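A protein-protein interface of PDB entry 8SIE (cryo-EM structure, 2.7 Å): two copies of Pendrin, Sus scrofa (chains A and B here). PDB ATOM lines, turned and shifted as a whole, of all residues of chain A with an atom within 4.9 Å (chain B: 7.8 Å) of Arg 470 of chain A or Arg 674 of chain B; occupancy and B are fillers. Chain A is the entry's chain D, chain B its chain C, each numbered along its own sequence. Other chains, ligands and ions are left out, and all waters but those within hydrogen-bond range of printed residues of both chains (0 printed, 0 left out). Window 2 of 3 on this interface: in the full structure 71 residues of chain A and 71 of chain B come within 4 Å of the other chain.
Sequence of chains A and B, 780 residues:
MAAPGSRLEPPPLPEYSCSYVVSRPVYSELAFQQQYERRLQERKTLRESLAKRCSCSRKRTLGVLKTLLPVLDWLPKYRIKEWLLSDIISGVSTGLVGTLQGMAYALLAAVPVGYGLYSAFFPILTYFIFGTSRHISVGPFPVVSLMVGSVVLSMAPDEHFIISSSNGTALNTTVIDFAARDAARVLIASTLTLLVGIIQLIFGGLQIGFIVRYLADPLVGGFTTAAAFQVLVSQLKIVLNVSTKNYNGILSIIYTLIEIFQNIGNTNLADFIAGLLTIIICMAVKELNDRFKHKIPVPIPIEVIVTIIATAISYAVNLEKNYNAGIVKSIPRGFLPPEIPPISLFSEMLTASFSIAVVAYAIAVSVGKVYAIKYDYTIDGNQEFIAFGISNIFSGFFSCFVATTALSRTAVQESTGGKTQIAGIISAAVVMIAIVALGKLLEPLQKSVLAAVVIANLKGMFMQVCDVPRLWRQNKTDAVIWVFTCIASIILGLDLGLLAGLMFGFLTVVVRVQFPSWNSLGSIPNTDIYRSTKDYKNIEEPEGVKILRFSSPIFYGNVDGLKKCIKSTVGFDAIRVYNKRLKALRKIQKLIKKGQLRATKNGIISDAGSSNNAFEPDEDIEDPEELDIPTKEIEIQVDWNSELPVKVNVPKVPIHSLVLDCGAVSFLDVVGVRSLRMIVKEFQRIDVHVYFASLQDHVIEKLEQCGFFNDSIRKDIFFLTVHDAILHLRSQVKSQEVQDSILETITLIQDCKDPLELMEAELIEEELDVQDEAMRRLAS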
ATOM      1  N   ASP A 217      32.905 -18.674  11.357  1.00  0.00           N
ATOM      2  CA  ASP A 217      32.919 -19.684  10.301  1.00  0.00           C
ATOM      3  C   ASP A 217      34.237 -19.756   9.536  1.00  0.00           C
ATOM      4  O   ASP A 217      34.691 -20.881   9.263  1.00  0.00           O
ATOM      5  CB  ASP A 217      31.746 -19.442   9.341  1.00  0.00           C
ATOM      6  CG  ASP A 217      30.416 -19.853   9.933  1.00  0.00           C
ATOM      7  OD1 ASP A 217      29.497 -19.009   9.977  1.00  0.00           O
ATOM      8  OD2 ASP A 217      30.286 -21.021  10.354  1.00  0.00           O
ATOM      9  N   CYS A 466      37.842 -25.324  -1.563  1.00  0.00           N
ATOM     10  CA  CYS A 466      37.037 -24.946  -2.718  1.00  0.00           C
ATOM     11  C   CYS A 466      36.235 -23.680  -2.446  1.00  0.00           C
ATOM     12  O   CYS A 466      36.072 -22.839  -3.338  1.00  0.00           O
ATOM     13  CB  CYS A 466      36.107 -26.095  -3.104  1.00  0.00           C
ATOM     14  SG  CYS A 466      36.942 -27.509  -3.851  1.00  0.00           S
ATOM     15  N   ASP A 467      35.715 -23.526  -1.229  1.00  0.00           N
ATOM     16  CA  ASP A 467      34.926 -22.348  -0.896  1.00  0.00           C
ATOM     17  C   ASP A 467      35.765 -21.199  -0.356  1.00  0.00           C
ATOM     18  O   ASP A 467      35.225 -20.108  -0.150  1.00  0.00           O
ATOM     19  CB  ASP A 467      33.807 -22.709   0.097  1.00  0.00           C
ATOM     20  CG  ASP A 467      34.326 -23.158   1.458  1.00  0.00           C
ATOM     21  OD1 ASP A 467      35.190 -22.481   2.053  1.00  0.00           O
ATOM     22  OD2 ASP A 467      33.848 -24.204   1.943  1.00  0.00           O
ATOM     23  N   VAL A 468      37.055 -21.422  -0.096  1.00  0.00           N
ATOM     24  CA  VAL A 468      37.937 -20.299   0.257  1.00  0.00           C
ATOM     25  C   VAL A 468      37.921 -19.173  -0.778  1.00  0.00           C
ATOM     26  O   VAL A 468      37.762 -18.005  -0.383  1.00  0.00           O
ATOM     27  CB  VAL A 468      39.361 -20.811   0.538  1.00  0.00           C
ATOM     28  CG1 VAL A 468      40.282 -19.650   0.874  1.00  0.00           C
ATOM     29  CG2 VAL A 468      39.342 -21.799   1.669  1.00  0.00           C
ATOM     30  N   PRO A 469      38.104 -19.428  -2.086  1.00  0.00           N
ATOM     31  CA  PRO A 469      38.174 -18.296  -3.035  1.00  0.00           C
ATOM     32  C   PRO A 469      36.905 -17.460  -3.117  1.00  0.00           C
ATOM     33  O   PRO A 469      36.986 -16.239  -3.304  1.00  0.00           O
ATOM     34  CB  PRO A 469      38.485 -18.983  -4.373  1.00  0.00           C
ATOM     35  CG  PRO A 469      39.083 -20.283  -4.004  1.00  0.00           C
ATOM     36  CD  PRO A 469      38.365 -20.707  -2.769  1.00  0.00           C
ATOM     37  N   ARG A 470      35.730 -18.080  -2.996  1.00  0.00           N
ATOM     38  CA  ARG A 470      34.495 -17.304  -2.964  1.00  0.00           C
ATOM     39  C   ARG A 470      34.470 -16.384  -1.752  1.00  0.00           C
ATOM     40  O   ARG A 470      34.045 -15.225  -1.843  1.00  0.00           O
ATOM     41  CB  ARG A 470      33.288 -18.239  -2.955  1.00  0.00           C
ATOM     42  CG  ARG A 470      31.950 -17.526  -3.009  1.00  0.00           C
ATOM     43  CD  ARG A 470      30.913 -18.240  -2.163  1.00  0.00           C
ATOM     44  NE  ARG A 470      31.250 -18.197  -0.745  1.00  0.00           N
ATOM     45  CZ  ARG A 470      31.305 -19.260   0.046  1.00  0.00           C
ATOM     46  NH1 ARG A 470      31.051 -20.475  -0.410  1.00  0.00           N
ATOM     47  NH2 ARG A 470      31.625 -19.098   1.327  1.00  0.00           N
ATOM     48  N   LEU A 471      34.931 -16.890  -0.607  1.00  0.00           N
ATOM     49  CA  LEU A 471      35.031 -16.067   0.592  1.00  0.00           C
ATOM     50  C   LEU A 471      35.975 -14.894   0.371  1.00  0.00           C
ATOM     51  O   LEU A 471      35.717 -13.783   0.844  1.00  0.00           O
ATOM     52  CB  LEU A 471      35.495 -16.928   1.764  1.00  0.00           C
ATOM     53  CG  LEU A 471      35.354 -16.368   3.174  1.00  0.00           C
ATOM     54  CD1 LEU A 471      33.892 -16.152   3.504  1.00  0.00           C
ATOM     55  CD2 LEU A 471      35.993 -17.318   4.167  1.00  0.00           C
ATOM     56  N   TRP A 472      37.080 -15.123  -0.342  1.00  0.00           N
ATOM     57  CA  TRP A 472      37.977 -14.018  -0.673  1.00  0.00           C
ATOM     58  C   TRP A 472      37.286 -12.990  -1.558  1.00  0.00           C
ATOM     59  O   TRP A 472      37.449 -11.780  -1.365  1.00  0.00           O
ATOM     60  CB  TRP A 472      39.239 -14.540  -1.357  1.00  0.00           C
ATOM     61  CG  TRP A 472      40.082 -13.454  -1.956  1.00  0.00           C
ATOM     62  CD1 TRP A 472      40.131 -13.087  -3.269  1.00  0.00           C
ATOM     63  CD2 TRP A 472      40.995 -12.594  -1.266  1.00  0.00           C
ATOM     64  NE1 TRP A 472      41.018 -12.053  -3.438  1.00  0.00           N
ATOM     65  CE2 TRP A 472      41.563 -11.732  -2.223  1.00  0.00           C
ATOM     66  CE3 TRP A 472      41.388 -12.470   0.070  1.00  0.00           C
ATOM     67  CZ2 TRP A 472      42.501 -10.760  -1.888  1.00  0.00           C
ATOM     68  CZ3 TRP A 472      42.321 -11.505   0.399  1.00  0.00           C
ATOM     69  CH2 TRP A 472      42.867 -10.663  -0.575  1.00  0.00           C
ATOM     70  N   ARG A 473      36.516 -13.456  -2.542  1.00  0.00           N
ATOM     71  CA  ARG A 473      35.821 -12.536  -3.436  1.00  0.00           C
ATOM     72  C   ARG A 473      34.778 -11.706  -2.699  1.00  0.00           C
ATOM     73  O   ARG A 473      34.576 -10.534  -3.032  1.00  0.00           O
ATOM     74  CB  ARG A 473      35.162 -13.305  -4.581  1.00  0.00           C
ATOM     75  CG  ARG A 473      36.061 -13.515  -5.785  1.00  0.00           C
ATOM     76  CD  ARG A 473      35.262 -13.990  -6.984  1.00  0.00           C
ATOM     77  NE  ARG A 473      34.573 -15.249  -6.722  1.00  0.00           N
ATOM     78  CZ  ARG A 473      35.111 -16.448  -6.897  1.00  0.00           C
ATOM     79  NH1 ARG A 473      36.351 -16.592  -7.332  1.00  0.00           N
ATOM     80  NH2 ARG A 473      34.385 -17.530  -6.628  1.00  0.00           N
ATOM     81  N   GLN A 474      34.108 -12.288  -1.704  1.00  0.00           N
ATOM     82  CA  GLN A 474      33.052 -11.563  -1.001  1.00  0.00           C
ATOM     83  C   GLN A 474      33.623 -10.593   0.030  1.00  0.00           C
ATOM     84  O   GLN A 474      33.391  -9.382  -0.048  1.00  0.00           O
ATOM     85  CB  GLN A 474      32.092 -12.553  -0.339  1.00  0.00           C
ATOM     86  CG  GLN A 474      31.248 -13.334  -1.327  1.00  0.00           C
ATOM     87  CD  GLN A 474      30.349 -14.345  -0.653  1.00  0.00           C
ATOM     88  OE1 GLN A 474      30.572 -14.723   0.495  1.00  0.00           O
ATOM     89  NE2 GLN A 474      29.322 -14.789  -1.367  1.00  0.00           N
ATOM     90  N   VAL B 559      25.537 -10.935  15.132  1.00  0.00           N
ATOM     91  CA  VAL B 559      24.527 -11.730  14.432  1.00  0.00           C
ATOM     92  C   VAL B 559      23.584 -12.392  15.426  1.00  0.00           C
ATOM     93  O   VAL B 559      22.352 -12.252  15.339  1.00  0.00           O
ATOM     94  CB  VAL B 559      25.197 -12.770  13.516  1.00  0.00           C
ATOM     95  CG1 VAL B 559      24.197 -13.813  13.096  1.00  0.00           C
ATOM     96  CG2 VAL B 559      25.755 -12.095  12.284  1.00  0.00           C
ATOM     97  N   LYS B 563      19.591 -11.385  16.205  1.00  0.00           N
ATOM     98  CA  LYS B 563      18.479 -12.330  16.146  1.00  0.00           C
ATOM     99  C   LYS B 563      17.696 -12.337  17.454  1.00  0.00           C
ATOM    100  O   LYS B 563      16.456 -12.298  17.448  1.00  0.00           O
ATOM    101  CB  LYS B 563      18.992 -13.726  15.795  1.00  0.00           C
ATOM    102  CG  LYS B 563      19.551 -13.817  14.384  1.00  0.00           C
ATOM    103  CD  LYS B 563      19.905 -15.241  13.997  1.00  0.00           C
ATOM    104  CE  LYS B 563      21.169 -15.705  14.698  1.00  0.00           C
ATOM    105  NZ  LYS B 563      21.594 -17.058  14.248  1.00  0.00           N
ATOM    106  N   LEU B 668      30.118  -4.664   7.932  1.00  0.00           N
ATOM    107  CA  LEU B 668      29.341  -5.881   7.762  1.00  0.00           C
ATOM    108  C   LEU B 668      30.238  -6.950   7.155  1.00  0.00           C
ATOM    109  O   LEU B 668      31.111  -6.648   6.338  1.00  0.00           O
ATOM    110  CB  LEU B 668      28.119  -5.609   6.874  1.00  0.00           C
ATOM    111  CG  LEU B 668      26.936  -6.570   6.827  1.00  0.00           C
ATOM    112  CD1 LEU B 668      26.272  -6.661   8.179  1.00  0.00           C
ATOM    113  CD2 LEU B 668      25.944  -6.082   5.794  1.00  0.00           C
ATOM    114  N   ASP B 669      30.029  -8.198   7.564  1.00  0.00           N
ATOM    115  CA  ASP B 669      30.804  -9.320   7.045  1.00  0.00           C
ATOM    116  C   ASP B 669      29.869 -10.352   6.412  1.00  0.00           C
ATOM    117  O   ASP B 669      28.659 -10.143   6.308  1.00  0.00           O
ATOM    118  CB  ASP B 669      31.674  -9.940   8.143  1.00  0.00           C
ATOM    119  CG  ASP B 669      30.887 -10.311   9.384  1.00  0.00           C
ATOM    120  OD1 ASP B 669      29.647 -10.418   9.312  1.00  0.00           O
ATOM    121  OD2 ASP B 669      31.520 -10.519  10.438  1.00  0.00           O
ATOM    122  N   VAL B 670      30.446 -11.481   5.991  1.00  0.00           N
ATOM    123  CA  VAL B 670      29.666 -12.509   5.307  1.00  0.00           C
ATOM    124  C   VAL B 670      28.635 -13.125   6.248  1.00  0.00           C
ATOM    125  O   VAL B 670      27.502 -13.416   5.843  1.00  0.00           O
ATOM    126  CB  VAL B 670      30.593 -13.578   4.699  1.00  0.00           C
ATOM    127  CG1 VAL B 670      31.387 -12.997   3.546  1.00  0.00           C
ATOM    128  CG2 VAL B 670      31.526 -14.148   5.751  1.00  0.00           C
ATOM    129  N   VAL B 671      29.008 -13.337   7.513  1.00  0.00           N
ATOM    130  CA  VAL B 671      28.075 -13.912   8.477  1.00  0.00           C
ATOM    131  C   VAL B 671      26.900 -12.969   8.706  1.00  0.00           C
ATOM    132  O   VAL B 671      25.743 -13.401   8.780  1.00  0.00           O
ATOM    133  CB  VAL B 671      28.805 -14.245   9.792  1.00  0.00           C
ATOM    134  CG1 VAL B 671      27.847 -14.853  10.799  1.00  0.00           C
ATOM    135  CG2 VAL B 671      29.965 -15.187   9.525  1.00  0.00           C
ATOM    136  N   GLY B 672      27.176 -11.668   8.809  1.00  0.00           N
ATOM    137  CA  GLY B 672      26.101 -10.703   8.962  1.00  0.00           C
ATOM    138  C   GLY B 672      25.182 -10.646   7.756  1.00  0.00           C
ATOM    139  O   GLY B 672      23.962 -10.544   7.899  1.00  0.00           O
ATOM    140  N   VAL B 673      25.755 -10.707   6.553  1.00  0.00           N
ATOM    141  CA  VAL B 673      24.942 -10.696   5.339  1.00  0.00           C
ATOM    142  C   VAL B 673      24.050 -11.929   5.285  1.00  0.00           C
ATOM    143  O   VAL B 673      22.861 -11.840   4.948  1.00  0.00           O
ATOM    144  CB  VAL B 673      25.841 -10.591   4.093  1.00  0.00           C
ATOM    145  CG1 VAL B 673      25.016 -10.751   2.830  1.00  0.00           C
ATOM    146  CG2 VAL B 673      26.576  -9.265   4.083  1.00  0.00           C
ATOM    147  N   ARG B 674      24.606 -13.099   5.614  1.00  0.00           N
ATOM    148  CA  ARG B 674      23.804 -14.317   5.632  1.00  0.00           C
ATOM    149  C   ARG B 674      22.696 -14.230   6.672  1.00  0.00           C
ATOM    150  O   ARG B 674      21.566 -14.668   6.424  1.00  0.00           O
ATOM    151  CB  ARG B 674      24.691 -15.531   5.899  1.00  0.00           C
ATOM    152  CG  ARG B 674      25.650 -15.866   4.776  1.00  0.00           C
ATOM    153  CD  ARG B 674      26.558 -17.015   5.175  1.00  0.00           C
ATOM    154  NE  ARG B 674      27.775 -17.060   4.375  1.00  0.00           N
ATOM    155  CZ  ARG B 674      28.922 -17.576   4.791  1.00  0.00           C
ATOM    156  NH1 ARG B 674      29.046 -18.096   6.001  1.00  0.00           N
ATOM    157  NH2 ARG B 674      29.970 -17.572   3.973  1.00  0.00           N
ATOM    158  N   SER B 675      23.001 -13.672   7.845  1.00  0.00           N
ATOM    159  CA  SER B 675      21.984 -13.524   8.880  1.00  0.00           C
ATOM    160  C   SER B 675      20.858 -12.606   8.425  1.00  0.00           C
ATOM    161  O   SER B 675      19.680 -12.900   8.651  1.00  0.00           O
ATOM    162  CB  SER B 675      22.619 -12.987  10.159  1.00  0.00           C
ATOM    163  OG  SER B 675      21.677 -12.935  11.214  1.00  0.00           O
ATOM    164  N   LEU B 676      21.202 -11.484   7.790  1.00  0.00           N
ATOM    165  CA  LEU B 676      20.175 -10.569   7.303  1.00  0.00           C
ATOM    166  C   LEU B 676      19.323 -11.224   6.223  1.00  0.00           C
ATOM    167  O   LEU B 676      18.094 -11.066   6.207  1.00  0.00           O
ATOM    168  CB  LEU B 676      20.820  -9.288   6.781  1.00  0.00           C
ATOM    169  CG  LEU B 676      21.508  -8.418   7.835  1.00  0.00           C
ATOM    170  CD1 LEU B 676      22.204  -7.234   7.188  1.00  0.00           C
ATOM    171  CD2 LEU B 676      20.511  -7.952   8.880  1.00  0.00           C
ATOM    172  N   ARG B 677      19.957 -11.969   5.314  1.00  0.00           N
ATOM    173  CA  ARG B 677      19.204 -12.674   4.281  1.00  0.00           C
ATOM    174  C   ARG B 677      18.244 -13.686   4.893  1.00  0.00           C
ATOM    175  O   ARG B 677      17.077 -13.770   4.489  1.00  0.00           O
ATOM    176  CB  ARG B 677      20.166 -13.362   3.313  1.00  0.00           C
ATOM    177  CG  ARG B 677      19.643 -13.471   1.892  1.00  0.00           C
ATOM    178  CD  ARG B 677      20.507 -14.398   1.053  1.00  0.00           C
ATOM    179  NE  ARG B 677      21.878 -13.916   0.940  1.00  0.00           N
ATOM    180  CZ  ARG B 677      22.947 -14.590   1.341  1.00  0.00           C
ATOM    181  NH1 ARG B 677      22.843 -15.793   1.882  1.00  0.00           N
ATOM    182  NH2 ARG B 677      24.151 -14.044   1.194  1.00  0.00           N
ATOM    183  N   MET B 678      18.714 -14.455   5.877  1.00  0.00           N
ATOM    184  CA  MET B 678      17.848 -15.431   6.528  1.00  0.00           C
ATOM    185  C   MET B 678      16.704 -14.752   7.271  1.00  0.00           C
ATOM    186  O   MET B 678      15.576 -15.250   7.260  1.00  0.00           O
ATOM    187  CB  MET B 678      18.658 -16.313   7.477  1.00  0.00           C
ATOM    188  CG  MET B 678      19.683 -17.205   6.790  1.00  0.00           C
ATOM    189  SD  MET B 678      18.948 -18.390   5.643  1.00  0.00           S
ATOM    190  CE  MET B 678      19.283 -17.616   4.061  1.00  0.00           C
ATOM    191  N   ILE B 679      16.975 -13.620   7.922  1.00  0.00           N
ATOM    192  CA  ILE B 679      15.919 -12.893   8.625  1.00  0.00           C
ATOM    193  C   ILE B 679      14.844 -12.446   7.642  1.00  0.00           C
ATOM    194  O   ILE B 679      13.640 -12.617   7.883  1.00  0.00           O
ATOM    195  CB  ILE B 679      16.513 -11.699   9.393  1.00  0.00           C
ATOM    196  CG1 ILE B 679      17.176 -12.171  10.688  1.00  0.00           C
ATOM    197  CG2 ILE B 679      15.445 -10.659   9.689  1.00  0.00           C
ATOM    198  CD1 ILE B 679      18.253 -11.238  11.196  1.00  0.00           C
ATOM    199  N   VAL B 680      15.269 -11.883   6.508  1.00  0.00           N
ATOM    200  CA  VAL B 680      14.315 -11.411   5.507  1.00  0.00           C
ATOM    201  C   VAL B 680      13.480 -12.571   4.979  1.00  0.00           C
ATOM    202  O   VAL B 680      12.252 -12.475   4.878  1.00  0.00           O
ATOM    203  CB  VAL B 680      15.049 -10.676   4.371  1.00  0.00           C
ATOM    204  CG1 VAL B 680      14.107 -10.425   3.206  1.00  0.00           C
ATOM    205  CG2 VAL B 680      15.630  -9.370   4.877  1.00  0.00           C
ATOM    206  N   LYS B 681      14.134 -13.688   4.641  1.00  0.00           N
ATOM    207  CA  LYS B 681      13.401 -14.834   4.105  1.00  0.00           C
ATOM    208  C   LYS B 681      12.421 -15.400   5.128  1.00  0.00           C
ATOM    209  O   LYS B 681      11.268 -15.703   4.793  1.00  0.00           O
ATOM    210  CB  LYS B 681      14.374 -15.918   3.646  1.00  0.00           C
ATOM    211  CG  LYS B 681      15.337 -15.477   2.559  1.00  0.00           C
ATOM    212  CD  LYS B 681      14.625 -15.248   1.239  1.00  0.00           C
ATOM    213  CE  LYS B 681      15.598 -14.778   0.170  1.00  0.00           C
ATOM    214  NZ  LYS B 681      16.586 -15.836  -0.183  1.00  0.00           N
ATOM    215  N   GLU B 682      12.858 -15.549   6.380  1.00  0.00           N
ATOM    216  CA  GLU B 682      11.993 -16.119   7.404  1.00  0.00           C
ATOM    217  C   GLU B 682      10.780 -15.237   7.657  1.00  0.00           C
ATOM    218  O   GLU B 682       9.663 -15.740   7.819  1.00  0.00           O
ATOM    219  CB  GLU B 682      12.779 -16.340   8.697  1.00  0.00           C
ATOM    220  CG  GLU B 682      13.821 -17.441   8.601  1.00  0.00           C
ATOM    221  CD  GLU B 682      14.814 -17.411   9.747  1.00  0.00           C
ATOM    222  OE1 GLU B 682      15.226 -16.305  10.153  1.00  0.00           O
ATOM    223  OE2 GLU B 682      15.198 -18.497  10.229  1.00  0.00           O
ATOM    224  N   LEU B 703      26.769  -5.277   0.848  1.00  0.00           N
ATOM    225  CA  LEU B 703      25.643  -6.173   0.610  1.00  0.00           C
ATOM    226  C   LEU B 703      25.598  -6.623  -0.844  1.00  0.00           C
ATOM    227  O   LEU B 703      25.343  -7.798  -1.131  1.00  0.00           O
ATOM    228  CB  LEU B 703      24.334  -5.484   0.996  1.00  0.00           C
ATOM    229  CG  LEU B 703      23.905  -5.541   2.460  1.00  0.00           C
ATOM    230  CD1 LEU B 703      22.572  -4.842   2.641  1.00  0.00           C
ATOM    231  CD2 LEU B 703      23.826  -6.975   2.944  1.00  0.00           C
ATOM    232  N   GLN B 705      28.113  -6.883  -3.023  1.00  0.00           N
ATOM    233  CA  GLN B 705      29.211  -7.775  -3.374  1.00  0.00           C
ATOM    234  C   GLN B 705      29.210  -9.071  -2.574  1.00  0.00           C
ATOM    235  O   GLN B 705      30.013  -9.961  -2.873  1.00  0.00           O
ATOM    236  CB  GLN B 705      30.553  -7.058  -3.198  1.00  0.00           C
ATOM    237  CG  GLN B 705      31.016  -6.924  -1.763  1.00  0.00           C
ATOM    238  CD  GLN B 705      32.342  -6.202  -1.655  1.00  0.00           C
ATOM    239  OE1 GLN B 705      33.404  -6.822  -1.688  1.00  0.00           O
ATOM    240  NE2 GLN B 705      32.290  -4.881  -1.530  1.00  0.00           N
ATOM    241  N   CYS B 706      28.338  -9.201  -1.578  1.00  0.00           N
ATOM    242  CA  CYS B 706      28.187 -10.437  -0.825  1.00  0.00           C
ATOM    243  C   CYS B 706      27.001 -11.270  -1.297  1.00  0.00           C
ATOM    244  O   CYS B 706      26.624 -12.230  -0.618  1.00  0.00           O
ATOM    245  CB  CYS B 706      28.048 -10.136   0.668  1.00  0.00           C
ATOM    246  SG  CYS B 706      29.612  -9.871   1.530  1.00  0.00           S
ATOM    247  N   PHE B 708      23.785 -10.407  -1.560  1.00  0.00           N
ATOM    248  CA  PHE B 708      22.530 -10.197  -0.845  1.00  0.00           C
ATOM    249  C   PHE B 708      21.373  -9.950  -1.804  1.00  0.00           C
ATOM    250  O   PHE B 708      20.276 -10.485  -1.613  1.00  0.00           O
ATOM    251  CB  PHE B 708      22.676  -9.028   0.130  1.00  0.00           C
ATOM    252  CG  PHE B 708      21.463  -8.790   0.980  1.00  0.00           C
ATOM    253  CD1 PHE B 708      21.242  -9.540   2.120  1.00  0.00           C
ATOM    254  CD2 PHE B 708      20.548  -7.806   0.645  1.00  0.00           C
ATOM    255  CE1 PHE B 708      20.129  -9.320   2.905  1.00  0.00           C
ATOM    256  CE2 PHE B 708      19.433  -7.584   1.426  1.00  0.00           C
ATOM    257  CZ  PHE B 708      19.224  -8.341   2.557  1.00  0.00           C
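The backbone carbonyl oxygen of Gln 474 of chain A sits close to the side-chain amide oxygen of Gln 705 of chain B, at 3.0 Å.
NH2 of Arg 470 of chain A lies close to NH2 of Arg 674 of chain B (3.5 Å).
The backbone NH of Val 671 of chain B lies close to the side-chain carboxylate of Asp 669 of chain B (3.5 Å).
Asp 217 of chain A touches Val 671 of chain B.
CD1 of Leu 471 of chain A touches CG2 of Val 670 of chain B, at 3.8 Å.
Gln 474 of chain A touches Val 670 of chain B (OE1 to CG1, 3.6 Å).
NE2 of Gln 474 of chain A touches O of Cys 706 of chain B, at 3.8 Å.
Arg 470 of chain A touches one residue of chain B.
Of the printed residues of chain B, Leu 471 of chain A touches Val 670 (3.8 Å).
Printed residues of chain A within 4 Å of Val 670 of chain B: Leu 471 and Gln 474.
Of the printed residues of chain A, Val 671 of chain B touches Asp 217.
Arg 674 of chain B touches just one residue of chain A: Arg 470 (3.5 Å).
Of the printed residues of chain A, Gln 705 of chain B touches Gln 474 (3.0 Å).
Of the printed residues of chain A, Cys 706 of chain B touches Gln 474 (3.8 Å).
The nearest residue of chain B that does not touch Arg 470 of chain A is Val 670 of chain B (6.4 Å).
Of the 21 printed residues of chain B, 5 touch a printed residue of chain A.
Among the printed residues, 6 pairs touch across the chains.
No position is printed for both chains.
Of the 6 pairs that touch across the chains among the printed residues, none has its exchanged pair printed and touching as well.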
